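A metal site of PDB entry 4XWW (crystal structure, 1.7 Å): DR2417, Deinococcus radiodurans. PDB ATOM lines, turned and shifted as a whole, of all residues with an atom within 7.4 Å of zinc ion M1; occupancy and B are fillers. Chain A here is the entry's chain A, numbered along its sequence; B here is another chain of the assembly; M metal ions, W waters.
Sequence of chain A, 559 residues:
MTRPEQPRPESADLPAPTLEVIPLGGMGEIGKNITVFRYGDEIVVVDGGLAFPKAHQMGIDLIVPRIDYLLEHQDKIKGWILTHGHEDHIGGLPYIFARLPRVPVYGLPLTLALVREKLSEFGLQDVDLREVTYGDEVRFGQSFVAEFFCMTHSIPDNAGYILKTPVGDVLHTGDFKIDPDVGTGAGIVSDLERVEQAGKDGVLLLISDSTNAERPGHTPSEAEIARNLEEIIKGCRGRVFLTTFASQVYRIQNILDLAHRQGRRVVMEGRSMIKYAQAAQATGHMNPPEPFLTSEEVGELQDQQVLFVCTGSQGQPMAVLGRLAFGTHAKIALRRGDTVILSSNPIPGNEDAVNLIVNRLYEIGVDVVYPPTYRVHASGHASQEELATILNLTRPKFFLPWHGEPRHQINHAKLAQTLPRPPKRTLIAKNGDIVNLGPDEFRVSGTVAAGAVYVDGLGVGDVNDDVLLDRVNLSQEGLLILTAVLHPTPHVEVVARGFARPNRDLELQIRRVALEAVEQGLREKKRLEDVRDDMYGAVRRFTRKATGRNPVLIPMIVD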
ATOM      1  N   ASN A  33      11.015 -11.800  30.204  1.00  0.00           N
ATOM      2  CA  ASN A  33      11.447 -10.709  29.358  1.00  0.00           C
ATOM      3  C   ASN A  33      11.346  -9.361  30.058  1.00  0.00           C
ATOM      4  O   ASN A  33      10.313  -9.031  30.654  1.00  0.00           O
ATOM      5  CB  ASN A  33      10.619 -10.726  28.081  1.00  0.00           C
ATOM      6  CG  ASN A  33      10.898 -11.961  27.249  1.00  0.00           C
ATOM      7  OD1 ASN A  33      11.931 -12.030  26.605  1.00  0.00           O
ATOM      8  ND2 ASN A  33      10.016 -12.939  27.287  1.00  0.00           N
ATOM      9  N   THR A  83       4.121  -5.137  25.762  1.00  0.00           N
ATOM     10  CA  THR A  83       3.869  -5.545  24.377  1.00  0.00           C
ATOM     11  C   THR A  83       2.673  -6.490  24.210  1.00  0.00           C
ATOM     12  O   THR A  83       1.994  -6.453  23.193  1.00  0.00           O
ATOM     13  CB  THR A  83       5.110  -6.211  23.716  1.00  0.00           C
ATOM     14  OG1 THR A  83       5.488  -7.393  24.434  1.00  0.00           O
ATOM     15  CG2 THR A  83       6.305  -5.231  23.658  1.00  0.00           C
ATOM     16  N   HIS A  84       2.433  -7.340  25.207  1.00  0.00           N
ATOM     17  CA  HIS A  84       1.309  -8.280  25.183  1.00  0.00           C
ATOM     18  C   HIS A  84       1.184  -8.980  26.539  1.00  0.00           C
ATOM     19  O   HIS A  84       2.081  -8.882  27.377  1.00  0.00           O
ATOM     20  CB  HIS A  84       1.425  -9.332  24.046  1.00  0.00           C
ATOM     21  CG  HIS A  84       2.583 -10.283  24.163  1.00  0.00           C
ATOM     22  ND1 HIS A  84       3.897  -9.896  24.069  1.00  0.00           N
ATOM     23  CD2 HIS A  84       2.609 -11.653  24.262  1.00  0.00           C
ATOM     24  CE1 HIS A  84       4.690 -10.960  24.130  1.00  0.00           C
ATOM     25  NE2 HIS A  84       3.920 -12.028  24.240  1.00  0.00           N
ATOM     26  N   GLY A  85       0.071  -9.670  26.739  1.00  0.00           N
ATOM     27  CA  GLY A  85      -0.291 -10.161  28.062  1.00  0.00           C
ATOM     28  C   GLY A  85       0.166 -11.592  28.382  1.00  0.00           C
ATOM     29  O   GLY A  85      -0.359 -12.186  29.328  1.00  0.00           O
ATOM     30  N   HIS A  86       1.111 -12.162  27.632  1.00  0.00           N
ATOM     31  CA  HIS A  86       1.679 -13.473  28.021  1.00  0.00           C
ATOM     32  C   HIS A  86       2.444 -13.370  29.330  1.00  0.00           C
ATOM     33  O   HIS A  86       3.049 -12.351  29.639  1.00  0.00           O
ATOM     34  CB  HIS A  86       2.620 -14.022  26.926  1.00  0.00           C
ATOM     35  CG  HIS A  86       1.918 -14.779  25.855  1.00  0.00           C
ATOM     36  ND1 HIS A  86       2.387 -14.840  24.556  1.00  0.00           N
ATOM     37  CD2 HIS A  86       0.765 -15.496  25.869  1.00  0.00           C
ATOM     38  CE1 HIS A  86       1.556 -15.563  23.822  1.00  0.00           C
ATOM     39  NE2 HIS A  86       0.575 -15.987  24.593  1.00  0.00           N
ATOM     40  N   GLU A  87       2.444 -14.457  30.111  1.00  0.00           N
ATOM     41  CA  GLU A  87       3.084 -14.466  31.413  1.00  0.00           C
ATOM     42  C   GLU A  87       4.583 -14.220  31.355  1.00  0.00           C
ATOM     43  O   GLU A  87       5.125 -13.694  32.301  1.00  0.00           O
ATOM     44  CB  GLU A  87       2.820 -15.792  32.133  1.00  0.00           C
ATOM     45  CG  GLU A  87       1.385 -15.911  32.669  1.00  0.00           C
ATOM     46  CD  GLU A  87       1.113 -15.070  33.890  1.00  0.00           C
ATOM     47  OE1 GLU A  87       2.050 -14.497  34.469  1.00  0.00           O
ATOM     48  OE2 GLU A  87      -0.066 -14.990  34.279  1.00  0.00           O
ATOM     49  N   ASP A  88       5.247 -14.582  30.264  1.00  0.00           N
ATOM     50  CA  ASP A  88       6.680 -14.282  30.221  1.00  0.00           C
ATOM     51  C   ASP A  88       6.952 -12.841  29.786  1.00  0.00           C
ATOM     52  O   ASP A  88       8.115 -12.461  29.581  1.00  0.00           O
ATOM     53  CB  ASP A  88       7.428 -15.261  29.301  1.00  0.00           C
ATOM     54  CG  ASP A  88       7.078 -15.095  27.850  1.00  0.00           C
ATOM     55  OD1 ASP A  88       5.868 -14.939  27.550  1.00  0.00           O
ATOM     56  OD2 ASP A  88       8.001 -15.140  27.017  1.00  0.00           O
ATOM     57  N   HIS A  89       5.902 -12.024  29.694  1.00  0.00           N
ATOM     58  CA  HIS A  89       6.075 -10.585  29.515  1.00  0.00           C
ATOM     59  C   HIS A  89       5.403  -9.745  30.595  1.00  0.00           C
ATOM     60  O   HIS A  89       5.821  -8.608  30.809  1.00  0.00           O
ATOM     61  CB  HIS A  89       5.594 -10.164  28.123  1.00  0.00           C
ATOM     62  CG  HIS A  89       6.345 -10.855  27.022  1.00  0.00           C
ATOM     63  ND1 HIS A  89       7.331 -10.220  26.287  1.00  0.00           N
ATOM     64  CD2 HIS A  89       6.300 -12.126  26.568  1.00  0.00           C
ATOM     65  CE1 HIS A  89       7.837 -11.073  25.410  1.00  0.00           C
ATOM     66  NE2 HIS A  89       7.228 -12.238  25.557  1.00  0.00           N
ATOM     67  N   HIS A 153       0.335 -12.923  16.769  1.00  0.00           N
ATOM     68  CA  HIS A 153       0.951 -13.762  17.797  1.00  0.00           C
ATOM     69  C   HIS A 153      -0.163 -14.684  18.295  1.00  0.00           C
ATOM     70  O   HIS A 153      -1.256 -14.698  17.729  1.00  0.00           O
ATOM     71  CB  HIS A 153       1.541 -12.861  18.903  1.00  0.00           C
ATOM     72  CG  HIS A 153       2.437 -13.564  19.886  1.00  0.00           C
ATOM     73  ND1 HIS A 153       3.173 -14.698  19.565  1.00  0.00           N
ATOM     74  CD2 HIS A 153       2.699 -13.301  21.189  1.00  0.00           C
ATOM     75  CE1 HIS A 153       3.848 -15.080  20.635  1.00  0.00           C
ATOM     76  NE2 HIS A 153       3.562 -14.271  21.628  1.00  0.00           N
ATOM     77  N   SER A 154       0.113 -15.427  19.360  1.00  0.00           N
ATOM     78  CA  SER A 154      -0.805 -16.436  19.870  1.00  0.00           C
ATOM     79  C   SER A 154      -1.742 -15.875  20.943  1.00  0.00           C
ATOM     80  O   SER A 154      -2.462 -16.630  21.601  1.00  0.00           O
ATOM     81  CB  SER A 154      -0.013 -17.601  20.432  1.00  0.00           C
ATOM     82  OG  SER A 154       1.053 -17.076  21.210  1.00  0.00           O
ATOM     83  N   ILE A 155      -1.678 -14.554  21.139  1.00  0.00           N
ATOM     84  CA  ILE A 155      -2.618 -13.832  22.019  1.00  0.00           C
ATOM     85  C   ILE A 155      -2.982 -12.520  21.301  1.00  0.00           C
ATOM     86  O   ILE A 155      -2.148 -11.973  20.571  1.00  0.00           O
ATOM     87  CB  ILE A 155      -2.001 -13.573  23.428  1.00  0.00           C
ATOM     88  CG1 ILE A 155      -3.074 -13.119  24.435  1.00  0.00           C
ATOM     89  CG2 ILE A 155      -0.873 -12.520  23.354  1.00  0.00           C
ATOM     90  CD1 ILE A 155      -2.540 -12.927  25.859  1.00  0.00           C
ATOM     91  N   ASN A 158      -1.286  -7.840  20.606  1.00  0.00           N
ATOM     92  CA  ASN A 158       0.160  -8.016  20.614  1.00  0.00           C
ATOM     93  C   ASN A 158       0.823  -6.970  19.741  1.00  0.00           C
ATOM     94  O   ASN A 158       0.440  -6.795  18.586  1.00  0.00           O
ATOM     95  CB  ASN A 158       0.513  -9.407  20.107  1.00  0.00           C
ATOM     96  CG  ASN A 158       1.995  -9.655  20.135  1.00  0.00           C
ATOM     97  OD1 ASN A 158       2.557  -9.915  21.191  1.00  0.00           O
ATOM     98  ND2 ASN A 158       2.627  -9.600  18.968  1.00  0.00           N
ATOM     99  N   GLY A 174       8.578  -7.379  18.933  1.00  0.00           N
ATOM    100  CA  GLY A 174       7.856  -8.125  19.945  1.00  0.00           C
ATOM    101  C   GLY A 174       7.928  -9.608  19.631  1.00  0.00           C
ATOM    102  O   GLY A 174       8.677 -10.042  18.756  1.00  0.00           O
ATOM    103  N   ASP A 175       7.152 -10.378  20.369  1.00  0.00           N
ATOM    104  CA  ASP A 175       6.955 -11.786  20.034  1.00  0.00           C
ATOM    105  C   ASP A 175       5.976 -11.834  18.880  1.00  0.00           C
ATOM    106  O   ASP A 175       4.935 -11.157  18.928  1.00  0.00           O
ATOM    107  CB  ASP A 175       6.439 -12.547  21.263  1.00  0.00           C
ATOM    108  N   PHE A 176       6.287 -12.584  17.830  1.00  0.00           N
ATOM    109  CA  PHE A 176       5.449 -12.560  16.642  1.00  0.00           C
ATOM    110  C   PHE A 176       5.542 -13.770  15.742  1.00  0.00           C
ATOM    111  O   PHE A 176       6.549 -14.488  15.741  1.00  0.00           O
ATOM    112  CB  PHE A 176       5.762 -11.328  15.771  1.00  0.00           C
ATOM    113  CG  PHE A 176       6.991 -11.501  14.897  1.00  0.00           C
ATOM    114  CD1 PHE A 176       8.257 -11.371  15.443  1.00  0.00           C
ATOM    115  CD2 PHE A 176       6.872 -11.773  13.547  1.00  0.00           C
ATOM    116  CE1 PHE A 176       9.402 -11.505  14.648  1.00  0.00           C
ATOM    117  CE2 PHE A 176       8.003 -11.901  12.733  1.00  0.00           C
ATOM    118  CZ  PHE A 176       9.276 -11.791  13.289  1.00  0.00           C
ATOM    119  N   ASP A 209      12.395 -11.652  17.517  1.00  0.00           N
ATOM    120  CA  ASP A 209      12.023 -12.875  18.223  1.00  0.00           C
ATOM    121  C   ASP A 209      12.706 -14.106  17.632  1.00  0.00           C
ATOM    122  O   ASP A 209      12.455 -14.465  16.496  1.00  0.00           O
ATOM    123  CB  ASP A 209      10.494 -12.988  18.134  1.00  0.00           C
ATOM    124  CG  ASP A 209       9.922 -14.231  18.797  1.00  0.00           C
ATOM    125  OD1 ASP A 209      10.658 -15.035  19.423  1.00  0.00           O
ATOM    126  OD2 ASP A 209       8.675 -14.374  18.704  1.00  0.00           O
ATOM    127  N   GLY A 380       2.925 -19.773  18.068  1.00  0.00           N
ATOM    128  CA  GLY A 380       2.757 -18.328  18.084  1.00  0.00           C
ATOM    129  C   GLY A 380       3.958 -17.591  17.506  1.00  0.00           C
ATOM    130  O   GLY A 380       3.936 -16.366  17.426  1.00  0.00           O
ATOM    131  N   HIS A 381       5.039 -18.307  17.162  1.00  0.00           N
ATOM    132  CA  HIS A 381       6.264 -17.589  16.775  1.00  0.00           C
ATOM    133  C   HIS A 381       6.712 -17.900  15.333  1.00  0.00           C
ATOM    134  O   HIS A 381       6.581 -19.011  14.829  1.00  0.00           O
ATOM    135  CB  HIS A 381       7.407 -17.893  17.749  1.00  0.00           C
ATOM    136  CG  HIS A 381       7.101 -17.569  19.182  1.00  0.00           C
ATOM    137  ND1 HIS A 381       7.445 -16.361  19.753  1.00  0.00           N
ATOM    138  CD2 HIS A 381       6.480 -18.286  20.149  1.00  0.00           C
ATOM    139  CE1 HIS A 381       7.073 -16.355  21.024  1.00  0.00           C
ATOM    140  NE2 HIS A 381       6.489 -17.509  21.287  1.00  0.00           N
ATOM    141  N   HIS A 403      14.756 -13.097  22.737  1.00  0.00           N
ATOM    142  CA  HIS A 403      13.719 -14.095  23.038  1.00  0.00           C
ATOM    143  C   HIS A 403      14.129 -15.489  22.554  1.00  0.00           C
ATOM    144  O   HIS A 403      13.423 -16.155  21.780  1.00  0.00           O
ATOM    145  CB  HIS A 403      12.359 -13.669  22.417  1.00  0.00           C
ATOM    146  CG  HIS A 403      11.146 -14.293  23.069  1.00  0.00           C
ATOM    147  ND1 HIS A 403      10.786 -15.601  22.830  1.00  0.00           N
ATOM    148  CD2 HIS A 403      10.196 -13.786  23.875  1.00  0.00           C
ATOM    149  CE1 HIS A 403       9.671 -15.881  23.487  1.00  0.00           C
ATOM    150  NE2 HIS A 403       9.294 -14.796  24.139  1.00  0.00           N
ATOM    151  P     U B   2       4.491 -22.311  20.554  1.00  0.00           P
ATOM    152  OP1   U B   2       3.375 -21.349  20.744  1.00  0.00           O
ATOM    153  OP2   U B   2       5.447 -22.114  19.437  1.00  0.00           O
ATOM    154  O5'   U B   2       5.364 -22.384  21.881  1.00  0.00           O
ATOM    155  C5'   U B   2       4.745 -22.526  23.173  1.00  0.00           C
ATOM    156  C4'   U B   2       5.530 -21.745  24.212  1.00  0.00           C
ATOM    157  O4'   U B   2       6.780 -22.423  24.511  1.00  0.00           O
ATOM    158  C3'   U B   2       5.908 -20.323  23.815  1.00  0.00           C
ATOM    159  O3'   U B   2       5.746 -19.473  24.941  1.00  0.00           O
ATOM    160  C2'   U B   2       7.403 -20.431  23.509  1.00  0.00           C
ATOM    161  O2'   U B   2       8.095 -19.211  23.681  1.00  0.00           O
ATOM    162  C1'   U B   2       7.826 -21.476  24.525  1.00  0.00           C
ATOM    163  N1    U B   2       9.081 -22.158  24.207  1.00  0.00           N
ATOM    164  C2    U B   2       9.976 -22.380  25.239  1.00  0.00           C
ATOM    165  O2    U B   2       9.752 -22.049  26.387  1.00  0.00           O
ATOM    166  N3    U B   2      11.138 -23.019  24.880  1.00  0.00           N
ATOM    167  C4    U B   2      11.498 -23.436  23.619  1.00  0.00           C
ATOM    168  O4    U B   2      12.580 -24.000  23.447  1.00  0.00           O
ATOM    169  C5    U B   2      10.527 -23.164  22.604  1.00  0.00           C
ATOM    170  C6    U B   2       9.378 -22.554  22.923  1.00  0.00           C
ATOM    171  P     U B   3       5.123 -18.016  24.761  1.00  0.00           P
ATOM    172  OP1   U B   3       4.757 -17.853  23.342  1.00  0.00           O
ATOM    173  OP2   U B   3       6.046 -17.047  25.406  1.00  0.00           O
ATOM    174  O5'   U B   3       3.775 -18.100  25.597  1.00  0.00           O
ATOM    175  C5'   U B   3       2.822 -19.130  25.334  1.00  0.00           C
ATOM    176  C4'   U B   3       2.295 -19.683  26.631  1.00  0.00           C
ATOM    177  O4'   U B   3       3.179 -20.739  27.104  1.00  0.00           O
ATOM    178  C3'   U B   3       2.180 -18.672  27.760  1.00  0.00           C
ATOM    179  O3'   U B   3       0.955 -18.848  28.455  1.00  0.00           O
ATOM    180  C2'   U B   3       3.364 -19.007  28.661  1.00  0.00           C
ATOM    181  O2'   U B   3       3.164 -18.685  30.019  1.00  0.00           O
ATOM    182  C1'   U B   3       3.473 -20.517  28.466  1.00  0.00           C
ATOM    183  N1    U B   3       4.806 -21.054  28.755  1.00  0.00           N
ATOM    184  C2    U B   3       4.899 -22.142  29.594  1.00  0.00           C
ATOM    185  O2    U B   3       3.930 -22.674  30.088  1.00  0.00           O
ATOM    186  N3    U B   3       6.185 -22.580  29.832  1.00  0.00           N
ATOM    187  C4    U B   3       7.352 -22.050  29.323  1.00  0.00           C
ATOM    188  O4    U B   3       8.427 -22.561  29.634  1.00  0.00           O
ATOM    189  C5    U B   3       7.168 -20.917  28.462  1.00  0.00           C
ATOM    190  C6    U B   3       5.931 -20.465  28.217  1.00  0.00           C
ATOM    191  P     U B   4       0.163 -17.589  29.008  1.00  0.00           P
ATOM    192  OP1   U B   4      -1.050 -17.407  28.172  1.00  0.00           O
ATOM    193  OP2   U B   4       1.115 -16.468  29.164  1.00  0.00           O
ATOM    194  O5'   U B   4      -0.352 -18.082  30.431  1.00  0.00           O
ATOM    195  C5'   U B   4       0.543 -18.703  31.368  1.00  0.00           C
ATOM    196  C4'   U B   4       0.378 -20.198  31.348  1.00  0.00           C
ATOM    197  O4'   U B   4       1.556 -20.805  31.945  1.00  0.00           O
ATOM    198  C3'   U B   4      -0.816 -20.759  32.116  1.00  0.00           C
ATOM    199  O3'   U B   4      -1.977 -20.843  31.301  1.00  0.00           O
ATOM    200  C2'   U B   4      -0.265 -22.083  32.649  1.00  0.00           C
ATOM    201  O2'   U B   4      -0.186 -23.100  31.687  1.00  0.00           O
ATOM    202  C1'   U B   4       1.160 -21.670  32.994  1.00  0.00           C
ATOM    203  N1    U B   4       1.277 -20.940  34.264  1.00  0.00           N
ATOM    204  C2    U B   4       1.726 -21.640  35.365  1.00  0.00           C
ATOM    205  O2    U B   4       2.030 -22.814  35.324  1.00  0.00           O
ATOM    206  N3    U B   4       1.803 -20.905  36.518  1.00  0.00           N
ATOM    207  C4    U B   4       1.487 -19.563  36.680  1.00  0.00           C
ATOM    208  O4    U B   4       1.612 -19.044  37.791  1.00  0.00           O
ATOM    209  C5    U B   4       1.023 -18.922  35.494  1.00  0.00           C
ATOM    210  C6    U B   4       0.933 -19.610  34.350  1.00  0.00           C
HETATM  211 ZN    ZN M   1       4.143 -14.088  23.703  1.00  0.00          ZN
HETATM  212 ZN    ZN M   2       7.384 -14.337  25.062  1.00  0.00          ZN
HETATM  213  O   HOH W   1       5.862 -14.805  23.813  1.00  0.00           O
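A ring nitrogen (ND1) of His 84 sits close to the side-chain amide oxygen (OD1) of Asn 158, 3.2 Å away. ND1 of His 84 is in hydrogen-bond range of OG1 of Thr 83 (3.0 Å). O of Gly 380 lies within hydrogen-bond range of ND1 of His 153 (2.8 Å). ND2 of Asn 158 is in hydrogen-bond range of O of Asp 175 (2.8 Å). OP1 of U 3 of chain B sits at hydrogen-bond distance from a ring nitrogen (NE2) of His 381 (2.7 Å).
CB of Asp 175 touches zinc ion M1, at 3.7 Å. U 3 of chain B touches zinc ion M1 (OP1 to ZN, 3.8 Å). Along chain A the residues within 4 Å of zinc ion M1 span positions 84 to 175. The nearest printed residue that does not touch zinc ion M1 is His 89 (4.05 Å).
Zinc ion M1 is bound by water W1 (1.9 Å), a ring nitrogen (ND1) of His 86 (2.1 Å), a ring nitrogen (NE2) of His 84 (2.1 Å) and a ring nitrogen (NE2) of His 153 (2.2 Å). Zinc ion M1 has four donor atoms within binding distance.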
